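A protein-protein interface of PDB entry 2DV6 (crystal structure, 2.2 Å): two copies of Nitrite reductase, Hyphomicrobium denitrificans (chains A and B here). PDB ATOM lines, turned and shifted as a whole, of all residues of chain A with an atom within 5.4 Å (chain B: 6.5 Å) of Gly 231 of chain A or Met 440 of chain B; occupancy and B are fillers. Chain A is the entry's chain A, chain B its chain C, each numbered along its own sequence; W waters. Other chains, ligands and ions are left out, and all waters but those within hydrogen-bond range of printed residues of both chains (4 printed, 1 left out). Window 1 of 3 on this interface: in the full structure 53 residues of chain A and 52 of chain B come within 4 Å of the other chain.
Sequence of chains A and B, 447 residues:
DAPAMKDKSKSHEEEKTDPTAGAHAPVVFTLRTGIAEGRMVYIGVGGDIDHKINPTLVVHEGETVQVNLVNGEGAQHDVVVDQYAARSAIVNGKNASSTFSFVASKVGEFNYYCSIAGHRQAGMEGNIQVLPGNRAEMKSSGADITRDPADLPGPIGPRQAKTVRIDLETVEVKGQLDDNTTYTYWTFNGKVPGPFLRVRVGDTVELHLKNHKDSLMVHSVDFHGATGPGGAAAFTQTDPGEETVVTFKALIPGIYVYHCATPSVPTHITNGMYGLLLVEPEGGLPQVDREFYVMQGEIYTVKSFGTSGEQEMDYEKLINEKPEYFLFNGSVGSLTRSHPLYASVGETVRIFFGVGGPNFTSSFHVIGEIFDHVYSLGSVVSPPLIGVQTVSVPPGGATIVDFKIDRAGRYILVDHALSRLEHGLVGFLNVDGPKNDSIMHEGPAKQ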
ATOM      1  N   VAL A 221      10.180   9.249   0.033  1.00  0.00           N
ATOM      2  CA  VAL A 221       9.534  10.441  -0.495  1.00  0.00           C
ATOM      3  C   VAL A 221       8.018  10.391  -0.227  1.00  0.00           C
ATOM      4  O   VAL A 221       7.407   9.345  -0.342  1.00  0.00           O
ATOM      5  CB  VAL A 221       9.855  10.652  -2.025  1.00  0.00           C
ATOM      6  CG1 VAL A 221       9.371   9.404  -2.903  1.00  0.00           C
ATOM      7  CG2 VAL A 221       9.213  11.959  -2.530  1.00  0.00           C
ATOM      8  N   ASP A 222       7.448  11.525   0.171  1.00  0.00           N
ATOM      9  CA  ASP A 222       6.006  11.758   0.351  1.00  0.00           C
ATOM     10  C   ASP A 222       5.692  12.897  -0.652  1.00  0.00           C
ATOM     11  O   ASP A 222       6.295  13.968  -0.543  1.00  0.00           O
ATOM     12  CB  ASP A 222       5.788  12.204   1.831  1.00  0.00           C
ATOM     13  CG  ASP A 222       4.372  12.807   2.138  1.00  0.00           C
ATOM     14  OD1 ASP A 222       4.086  12.992   3.356  1.00  0.00           O
ATOM     15  OD2 ASP A 222       3.540  13.097   1.228  1.00  0.00           O
ATOM     16  N   PHE A 223       4.810  12.659  -1.635  1.00  0.00           N
ATOM     17  CA  PHE A 223       4.328  13.719  -2.545  1.00  0.00           C
ATOM     18  C   PHE A 223       2.955  14.240  -2.082  1.00  0.00           C
ATOM     19  O   PHE A 223       2.015  13.430  -1.932  1.00  0.00           O
ATOM     20  CB  PHE A 223       4.172  13.221  -4.000  1.00  0.00           C
ATOM     21  CG  PHE A 223       5.431  12.645  -4.615  1.00  0.00           C
ATOM     22  CD1 PHE A 223       5.692  11.262  -4.562  1.00  0.00           C
ATOM     23  CD2 PHE A 223       6.327  13.464  -5.277  1.00  0.00           C
ATOM     24  CE1 PHE A 223       6.844  10.726  -5.148  1.00  0.00           C
ATOM     25  CE2 PHE A 223       7.472  12.951  -5.862  1.00  0.00           C
ATOM     26  CZ  PHE A 223       7.749  11.573  -5.782  1.00  0.00           C
ATOM     27  N   ALA A 226       0.223  13.184  -4.395  1.00  0.00           N
ATOM     28  CA  ALA A 226      -0.104  11.771  -4.441  1.00  0.00           C
ATOM     29  C   ALA A 226      -1.249  11.435  -3.476  1.00  0.00           C
ATOM     30  O   ALA A 226      -1.380  12.042  -2.386  1.00  0.00           O
ATOM     31  CB  ALA A 226       1.148  10.913  -4.143  1.00  0.00           C
ATOM     32  N   THR A 227      -2.088  10.484  -3.879  1.00  0.00           N
ATOM     33  CA  THR A 227      -3.224  10.040  -3.051  1.00  0.00           C
ATOM     34  C   THR A 227      -2.966   8.616  -2.575  1.00  0.00           C
ATOM     35  O   THR A 227      -2.852   7.703  -3.393  1.00  0.00           O
ATOM     36  CB  THR A 227      -4.544  10.072  -3.849  1.00  0.00           C
ATOM     37  OG1 THR A 227      -4.797  11.399  -4.286  1.00  0.00           O
ATOM     38  CG2 THR A 227      -5.708   9.616  -3.012  1.00  0.00           C
ATOM     39  N   GLY A 228      -2.856   8.415  -1.268  1.00  0.00           N
ATOM     40  CA  GLY A 228      -2.508   7.086  -0.764  1.00  0.00           C
ATOM     41  C   GLY A 228      -1.496   7.137   0.362  1.00  0.00           C
ATOM     42  O   GLY A 228      -0.929   8.188   0.605  1.00  0.00           O
ATOM     43  N   PRO A 229      -1.224   5.974   1.018  1.00  0.00           N
ATOM     44  CA  PRO A 229      -0.448   5.875   2.271  1.00  0.00           C
ATOM     45  C   PRO A 229       0.885   6.606   2.238  1.00  0.00           C
ATOM     46  O   PRO A 229       1.744   6.340   1.375  1.00  0.00           O
ATOM     47  CB  PRO A 229      -0.232   4.360   2.441  1.00  0.00           C
ATOM     48  CG  PRO A 229      -1.388   3.725   1.690  1.00  0.00           C
ATOM     49  CD  PRO A 229      -1.674   4.642   0.535  1.00  0.00           C
ATOM     50  N   GLY A 230       1.049   7.527   3.200  1.00  0.00           N
ATOM     51  CA  GLY A 230       2.251   8.354   3.306  1.00  0.00           C
ATOM     52  C   GLY A 230       2.541   9.246   2.100  1.00  0.00           C
ATOM     53  O   GLY A 230       3.663   9.711   1.927  1.00  0.00           O
ATOM     54  N   GLY A 231       1.549   9.495   1.247  1.00  0.00           N
ATOM     55  CA  GLY A 231       1.810  10.171  -0.023  1.00  0.00           C
ATOM     56  C   GLY A 231       2.845   9.450  -0.899  1.00  0.00           C
ATOM     57  O   GLY A 231       3.508  10.092  -1.702  1.00  0.00           O
ATOM     58  N   ALA A 232       2.963   8.121  -0.734  1.00  0.00           N
ATOM     59  CA  ALA A 232       3.953   7.239  -1.394  1.00  0.00           C
ATOM     60  C   ALA A 232       5.058   6.789  -0.433  1.00  0.00           C
ATOM     61  O   ALA A 232       5.846   5.873  -0.754  1.00  0.00           O
ATOM     62  CB  ALA A 232       4.562   7.844  -2.678  1.00  0.00           C
ATOM     63  N   ALA A 233       5.119   7.422   0.743  1.00  0.00           N
ATOM     64  CA  ALA A 233       6.172   7.116   1.695  1.00  0.00           C
ATOM     65  C   ALA A 233       6.096   5.689   2.226  1.00  0.00           C
ATOM     66  O   ALA A 233       7.133   5.092   2.568  1.00  0.00           O
ATOM     67  CB  ALA A 233       6.141   8.112   2.859  1.00  0.00           C
ATOM     68  N   PHE A 235       5.631   3.209   0.497  1.00  0.00           N
ATOM     69  CA  PHE A 235       6.147   2.335  -0.571  1.00  0.00           C
ATOM     70  C   PHE A 235       7.601   2.671  -0.890  1.00  0.00           C
ATOM     71  O   PHE A 235       8.222   2.027  -1.752  1.00  0.00           O
ATOM     72  CB  PHE A 235       5.329   2.551  -1.828  1.00  0.00           C
ATOM     73  CG  PHE A 235       3.867   2.191  -1.684  1.00  0.00           C
ATOM     74  CD1 PHE A 235       2.936   3.121  -1.210  1.00  0.00           C
ATOM     75  CD2 PHE A 235       3.407   0.903  -2.039  1.00  0.00           C
ATOM     76  CE1 PHE A 235       1.574   2.777  -1.073  1.00  0.00           C
ATOM     77  CE2 PHE A 235       2.039   0.571  -1.934  1.00  0.00           C
ATOM     78  CZ  PHE A 235       1.126   1.508  -1.445  1.00  0.00           C
ATOM     79  N   VAL A 246       7.361   2.779  -7.119  1.00  0.00           N
ATOM     80  CA  VAL A 246       5.987   2.986  -6.723  1.00  0.00           C
ATOM     81  C   VAL A 246       5.294   3.658  -7.903  1.00  0.00           C
ATOM     82  O   VAL A 246       5.890   4.515  -8.546  1.00  0.00           O
ATOM     83  CB  VAL A 246       5.865   3.843  -5.398  1.00  0.00           C
ATOM     84  CG1 VAL A 246       6.393   5.291  -5.588  1.00  0.00           C
ATOM     85  CG2 VAL A 246       4.448   3.911  -4.969  1.00  0.00           C
ATOM     86  N   THR A 247       4.066   3.242  -8.205  1.00  0.00           N
ATOM     87  CA  THR A 247       3.288   3.898  -9.254  1.00  0.00           C
ATOM     88  C   THR A 247       2.107   4.575  -8.595  1.00  0.00           C
ATOM     89  O   THR A 247       1.488   3.992  -7.713  1.00  0.00           O
ATOM     90  CB  THR A 247       2.795   2.851 -10.311  1.00  0.00           C
ATOM     91  OG1 THR A 247       3.936   2.248 -10.917  1.00  0.00           O
ATOM     92  CG2 THR A 247       1.925   3.489 -11.404  1.00  0.00           C
ATOM     93  N   PHE A 248       1.780   5.791  -9.003  1.00  0.00           N
ATOM     94  CA  PHE A 248       0.632   6.459  -8.407  1.00  0.00           C
ATOM     95  C   PHE A 248      -0.049   7.341  -9.417  1.00  0.00           C
ATOM     96  O   PHE A 248       0.594   7.835 -10.333  1.00  0.00           O
ATOM     97  CB  PHE A 248       0.996   7.238  -7.104  1.00  0.00           C
ATOM     98  CG  PHE A 248       1.951   8.392  -7.301  1.00  0.00           C
ATOM     99  CD1 PHE A 248       1.480   9.653  -7.678  1.00  0.00           C
ATOM    100  CD2 PHE A 248       3.304   8.230  -7.073  1.00  0.00           C
ATOM    101  CE1 PHE A 248       2.365  10.733  -7.853  1.00  0.00           C
ATOM    102  CE2 PHE A 248       4.200   9.309  -7.234  1.00  0.00           C
ATOM    103  CZ  PHE A 248       3.725  10.546  -7.651  1.00  0.00           C
ATOM    104  N   LYS A 249      -1.355   7.502  -9.274  1.00  0.00           N
ATOM    105  CA  LYS A 249      -2.106   8.439 -10.113  1.00  0.00           C
ATOM    106  C   LYS A 249      -2.096   9.871  -9.556  1.00  0.00           C
ATOM    107  O   LYS A 249      -2.196  10.083  -8.331  1.00  0.00           O
ATOM    108  CB  LYS A 249      -3.558   7.963 -10.321  1.00  0.00           C
ATOM    109  CG  LYS A 249      -3.676   6.760 -11.275  1.00  0.00           C
ATOM    110  CD  LYS A 249      -5.122   6.530 -11.743  1.00  0.00           C
ATOM    111  CE  LYS A 249      -5.452   7.299 -13.080  1.00  0.00           C
ATOM    112  NZ  LYS A 249      -5.182   6.492 -14.366  1.00  0.00           N
ATOM    113  N   ILE B 367      -1.632  13.790   5.503  1.00  0.00           N
ATOM    114  CA  ILE B 367      -0.637  13.058   4.712  1.00  0.00           C
ATOM    115  C   ILE B 367      -1.313  11.926   3.935  1.00  0.00           C
ATOM    116  O   ILE B 367      -2.002  11.078   4.526  1.00  0.00           O
ATOM    117  CB  ILE B 367       0.448  12.419   5.638  1.00  0.00           C
ATOM    118  CG1 ILE B 367       1.238  13.493   6.417  1.00  0.00           C
ATOM    119  CG2 ILE B 367       1.379  11.468   4.849  1.00  0.00           C
ATOM    120  CD1 ILE B 367       2.166  12.923   7.501  1.00  0.00           C
ATOM    121  N   GLY B 368      -1.119  11.919   2.616  1.00  0.00           N
ATOM    122  CA  GLY B 368      -1.708  10.904   1.768  1.00  0.00           C
ATOM    123  C   GLY B 368      -3.015  11.330   1.134  1.00  0.00           C
ATOM    124  O   GLY B 368      -3.544  10.624   0.291  1.00  0.00           O
ATOM    125  N   GLU B 369      -3.529  12.491   1.515  1.00  0.00           N
ATOM    126  CA  GLU B 369      -4.745  13.007   0.898  1.00  0.00           C
ATOM    127  C   GLU B 369      -4.626  14.476   0.510  1.00  0.00           C
ATOM    128  O   GLU B 369      -3.621  15.121   0.844  1.00  0.00           O
ATOM    129  CB  GLU B 369      -5.989  12.715   1.764  1.00  0.00           C
ATOM    130  CG  GLU B 369      -6.745  11.422   1.294  1.00  0.00           C
ATOM    131  CD  GLU B 369      -7.508  11.647  -0.044  1.00  0.00           C
ATOM    132  OE1 GLU B 369      -8.047  10.681  -0.645  1.00  0.00           O
ATOM    133  OE2 GLU B 369      -7.619  12.806  -0.497  1.00  0.00           O
ATOM    134  N   ARG B 407      -9.061   5.768  -1.637  1.00  0.00           N
ATOM    135  CA  ARG B 407      -8.528   4.443  -1.411  1.00  0.00           C
ATOM    136  C   ARG B 407      -8.074   4.288   0.032  1.00  0.00           C
ATOM    137  O   ARG B 407      -8.025   5.261   0.779  1.00  0.00           O
ATOM    138  CB  ARG B 407      -7.398   4.149  -2.402  1.00  0.00           C
ATOM    139  CG  ARG B 407      -6.200   5.167  -2.390  1.00  0.00           C
ATOM    140  CD  ARG B 407      -4.871   4.426  -2.623  1.00  0.00           C
ATOM    141  NE  ARG B 407      -4.600   3.569  -1.469  1.00  0.00           N
ATOM    142  CZ  ARG B 407      -3.729   2.554  -1.425  1.00  0.00           C
ATOM    143  NH1 ARG B 407      -3.578   1.870  -0.291  1.00  0.00           N
ATOM    144  NH2 ARG B 407      -3.016   2.208  -2.492  1.00  0.00           N
ATOM    145  N   PRO B 434      -7.001  -2.893   0.741  1.00  0.00           N
ATOM    146  CA  PRO B 434      -5.683  -3.399   0.273  1.00  0.00           C
ATOM    147  C   PRO B 434      -4.584  -2.312   0.199  1.00  0.00           C
ATOM    148  O   PRO B 434      -4.883  -1.134  -0.069  1.00  0.00           O
ATOM    149  CB  PRO B 434      -5.992  -3.980  -1.122  1.00  0.00           C
ATOM    150  CG  PRO B 434      -7.324  -3.402  -1.522  1.00  0.00           C
ATOM    151  CD  PRO B 434      -8.058  -2.997  -0.278  1.00  0.00           C
ATOM    152  N   LYS B 435      -3.339  -2.705   0.453  1.00  0.00           N
ATOM    153  CA  LYS B 435      -2.192  -1.817   0.245  1.00  0.00           C
ATOM    154  C   LYS B 435      -2.132  -1.337  -1.225  1.00  0.00           C
ATOM    155  O   LYS B 435      -2.044  -0.119  -1.506  1.00  0.00           O
ATOM    156  CB  LYS B 435      -0.875  -2.518   0.606  1.00  0.00           C
ATOM    157  CG  LYS B 435       0.308  -1.530   0.686  1.00  0.00           C
ATOM    158  CD  LYS B 435       1.669  -2.195   0.978  1.00  0.00           C
ATOM    159  CE  LYS B 435       2.731  -1.119   1.373  1.00  0.00           C
ATOM    160  NZ  LYS B 435       4.143  -1.663   1.441  1.00  0.00           N
ATOM    161  N   ASN B 436      -2.206  -2.310  -2.148  1.00  0.00           N
ATOM    162  CA  ASN B 436      -1.976  -2.059  -3.562  1.00  0.00           C
ATOM    163  C   ASN B 436      -3.263  -1.937  -4.356  1.00  0.00           C
ATOM    164  O   ASN B 436      -4.177  -2.772  -4.224  1.00  0.00           O
ATOM    165  CB  ASN B 436      -1.041  -3.122  -4.153  1.00  0.00           C
ATOM    166  CG  ASN B 436       0.377  -3.013  -3.593  1.00  0.00           C
ATOM    167  OD1 ASN B 436       1.025  -1.981  -3.754  1.00  0.00           O
ATOM    168  ND2 ASN B 436       0.867  -4.075  -2.948  1.00  0.00           N
ATOM    169  N   ASP B 437      -3.337  -0.887  -5.172  1.00  0.00           N
ATOM    170  CA  ASP B 437      -4.439  -0.706  -6.094  1.00  0.00           C
ATOM    171  C   ASP B 437      -4.012   0.181  -7.265  1.00  0.00           C
ATOM    172  O   ASP B 437      -2.825   0.526  -7.390  1.00  0.00           O
ATOM    173  CB  ASP B 437      -5.677  -0.150  -5.367  1.00  0.00           C
ATOM    174  CG  ASP B 437      -5.489   1.284  -4.862  1.00  0.00           C
ATOM    175  OD1 ASP B 437      -4.676   2.069  -5.409  1.00  0.00           O
ATOM    176  OD2 ASP B 437      -6.197   1.631  -3.892  1.00  0.00           O
ATOM    177  N   SER B 438      -4.971   0.564  -8.112  1.00  0.00           N
ATOM    178  CA  SER B 438      -4.650   1.324  -9.314  1.00  0.00           C
ATOM    179  C   SER B 438      -4.231   2.777  -9.036  1.00  0.00           C
ATOM    180  O   SER B 438      -3.521   3.393  -9.856  1.00  0.00           O
ATOM    181  CB  SER B 438      -5.815   1.281 -10.320  1.00  0.00           C
ATOM    182  OG  SER B 438      -6.987   1.873  -9.792  1.00  0.00           O
ATOM    183  N   ILE B 439      -4.672   3.326  -7.894  1.00  0.00           N
ATOM    184  CA  ILE B 439      -4.327   4.700  -7.526  1.00  0.00           C
ATOM    185  C   ILE B 439      -2.893   4.808  -6.962  1.00  0.00           C
ATOM    186  O   ILE B 439      -2.228   5.825  -7.125  1.00  0.00           O
ATOM    187  CB  ILE B 439      -5.388   5.290  -6.588  1.00  0.00           C
ATOM    188  CG1 ILE B 439      -6.711   5.395  -7.357  1.00  0.00           C
ATOM    189  CG2 ILE B 439      -4.958   6.688  -6.059  1.00  0.00           C
ATOM    190  CD1 ILE B 439      -7.929   5.663  -6.507  1.00  0.00           C
ATOM    191  N   MET B 440      -2.420   3.748  -6.310  1.00  0.00           N
ATOM    192  CA  MET B 440      -1.043   3.696  -5.798  1.00  0.00           C
ATOM    193  C   MET B 440      -0.701   2.258  -5.484  1.00  0.00           C
ATOM    194  O   MET B 440      -1.411   1.621  -4.732  1.00  0.00           O
ATOM    195  CB  MET B 440      -0.882   4.562  -4.516  1.00  0.00           C
ATOM    196  CG  MET B 440       0.533   4.600  -3.939  1.00  0.00           C
ATOM    197  SD  MET B 440       0.768   5.685  -2.494  1.00  0.00           S
ATOM    198  CE  MET B 440       0.586   7.326  -3.243  1.00  0.00           C
ATOM    199  N   HIS B 441       0.405   1.764  -6.024  1.00  0.00           N
ATOM    200  CA  HIS B 441       0.834   0.392  -5.769  1.00  0.00           C
ATOM    201  C   HIS B 441       2.332   0.319  -5.872  1.00  0.00           C
ATOM    202  O   HIS B 441       2.941   1.164  -6.522  1.00  0.00           O
ATOM    203  CB  HIS B 441       0.188  -0.629  -6.758  1.00  0.00           C
ATOM    204  CG  HIS B 441       0.521  -0.394  -8.211  1.00  0.00           C
ATOM    205  ND1 HIS B 441       1.660  -0.901  -8.817  1.00  0.00           N
ATOM    206  CD2 HIS B 441      -0.158   0.263  -9.184  1.00  0.00           C
ATOM    207  CE1 HIS B 441       1.674  -0.551 -10.094  1.00  0.00           C
ATOM    208  NE2 HIS B 441       0.585   0.165 -10.340  1.00  0.00           N
ATOM    209  N   GLU B 442       2.920  -0.693  -5.235  1.00  0.00           N
ATOM    210  CA  GLU B 442       4.336  -0.975  -5.396  1.00  0.00           C
ATOM    211  C   GLU B 442       4.650  -1.502  -6.813  1.00  0.00           C
ATOM    212  O   GLU B 442       3.772  -2.043  -7.482  1.00  0.00           O
ATOM    213  CB  GLU B 442       4.818  -1.944  -4.325  1.00  0.00           C
ATOM    214  CG  GLU B 442       4.272  -3.360  -4.452  1.00  0.00           C
ATOM    215  CD  GLU B 442       4.726  -4.268  -3.290  1.00  0.00           C
ATOM    216  OE1 GLU B 442       5.945  -4.588  -3.237  1.00  0.00           O
ATOM    217  OE2 GLU B 442       3.865  -4.650  -2.442  1.00  0.00           O
HETATM  218  O   HOH W   1      -0.824   8.601   4.860  1.00  0.00           O
HETATM  219  O   HOH W   2       0.891  13.851   1.607  1.00  0.00           O
HETATM  220  O   HOH W   3      -7.089  12.684  -3.805  1.00  0.00           O
HETATM  221  O   HOH W   4      -1.959   8.775  -5.978  1.00  0.00           O
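Water W3 bridges the side-chain hydroxyl (OG1) of Thr 227 of chain A and the side-chain carboxylate (OE2) of Glu 369 of chain B. Water W4 lies within hydrogen-bond range of O of Lys 249 of chain A (2.7 Å), N of Thr 227 of chain A (2.7 Å) and O of Ile 439 of chain B (3.2 Å). Water W1 bridges N of Gly 230 of chain A (2.7 Å) and O of Ile 367 of chain B (2.8 Å). Water W2 bridges OD2 of Asp 222 of chain A (2.8 Å) and N of Gly 368 of chain B (3.0 Å).
N of Gly 228 of chain A sits at hydrogen-bond distance from O of Gly 368 of chain B (2.8 Å). The backbone NH (N) of Ala 232 of chain A sits close to the side-chain sulfur (SD) of Met 440 of chain B (3.7 Å). The backbone carbonyl oxygen of His 441 of chain B sits at hydrogen-bond distance from the backbone NH of Thr 247 of chain A (2.9 Å). The backbone NH of Lys 249 of chain A is in hydrogen-bond range of the backbone carbonyl oxygen of Ile 439 of chain B (2.9 Å).
Gly 231 of chain A touches two residues of chain B. Printed residues of chain A within 4 Å of Met 440 of chain B: Ala 226 (3.7 Å), Thr 227 (3.5 Å), Gly 228 (3.9 Å), Gly 231 (3.9 Å), Ala 232 (3.5 Å), Phe 235 (3.3 Å), Thr 247 (3.2 Å) and Phe 248 (3.9 Å). Of the printed residues of chain B, Lys 249 of chain A touches Ser 438 (3.7 Å) and Ile 439 (2.9 Å). Of the printed residues of chain A, Ser 438 of chain B touches Lys 249 (3.7 Å). Of the printed residues of chain B, Thr 247 of chain A touches Met 440 (3.2 Å) and His 441 (2.9 Å). Of the printed residues of chain B, Ala 232 of chain A touches Met 440. The nearest residue of chain B that does not touch Gly 231 of chain A is Ile 367 of chain B (4.1 Å).
The backbone carbonyl oxygen (O) of Gly 231 of chain A sits at hydrogen-bond distance from the backbone NH (N) of Phe 223 of chain A (2.9 Å). The guanidinium group (NH2) of Arg 407 of chain B sits at hydrogen-bond distance from the backbone carbonyl oxygen (O) of Lys 435 of chain B (2.7 Å). The guanidinium group of Arg 407 of chain B lies within salt-bridge range of the side-chain carboxylate of Asp 437 of chain B (3.4 Å). The backbone carbonyl oxygen (O) of Met 440 of chain B sits at hydrogen-bond distance from the guanidinium group (NH2) of Arg 407 of chain B. The side-chain amide oxygen of Asn 436 of chain B lies within hydrogen-bond range of the backbone NH of Glu 442 of chain B (2.7 Å). OD1 of Asp 437 of chain B lies within hydrogen-bond range of N of Met 440 of chain B, 3.0 Å away.
Of the 13 printed residues of chain B, 11 touch a printed residue of chain A. Hydrophobic or aromatic side chains of chain B that line the printed part of chain A: Ile 367, Ile 439, Met 440 and His 441. Of the 16 printed residues of chain A, 13 touch a printed residue of chain B. Hydrophobic or aromatic side chains of chain A that line the printed part of chain B: Ala 226, Pro 229, Phe 235, Val 246 and Phe 248. Along chain A the printed residues that touch a printed residue of chain B span positions 222 to 249.
No position is printed for both chains.
OD1 of Asp 222 of chain A touches CG2 of Ile 367 of chain B, 3.4 Å away. CG2 of Thr 227 of chain A touches OE1 of Glu 369 of chain B, at 3.5 Å. Thr 227 of chain A touches Ile 439 of chain B (O to CG2, 3.5 Å). Thr 227 of chain A touches Met 440 of chain B (O to CE, 3.5 Å). Arg 407 of chain B touches Pro 229 of chain A (NH1 to CD, 3.5 Å). N of Gly 231 of chain A touches CA of Gly 368 of chain B, 3.6 Å away. CE of Met 440 of chain B touches C of Gly 231 of chain A, at 3.9 Å. Lys 435 of chain B touches Phe 235 of chain A. CE2 of Phe 235 of chain A touches OD1 of Asn 436 of chain B, 3.3 Å away. Phe 235 of chain A touches Glu 442 of chain B (CD2 to N, 3.6 Å).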
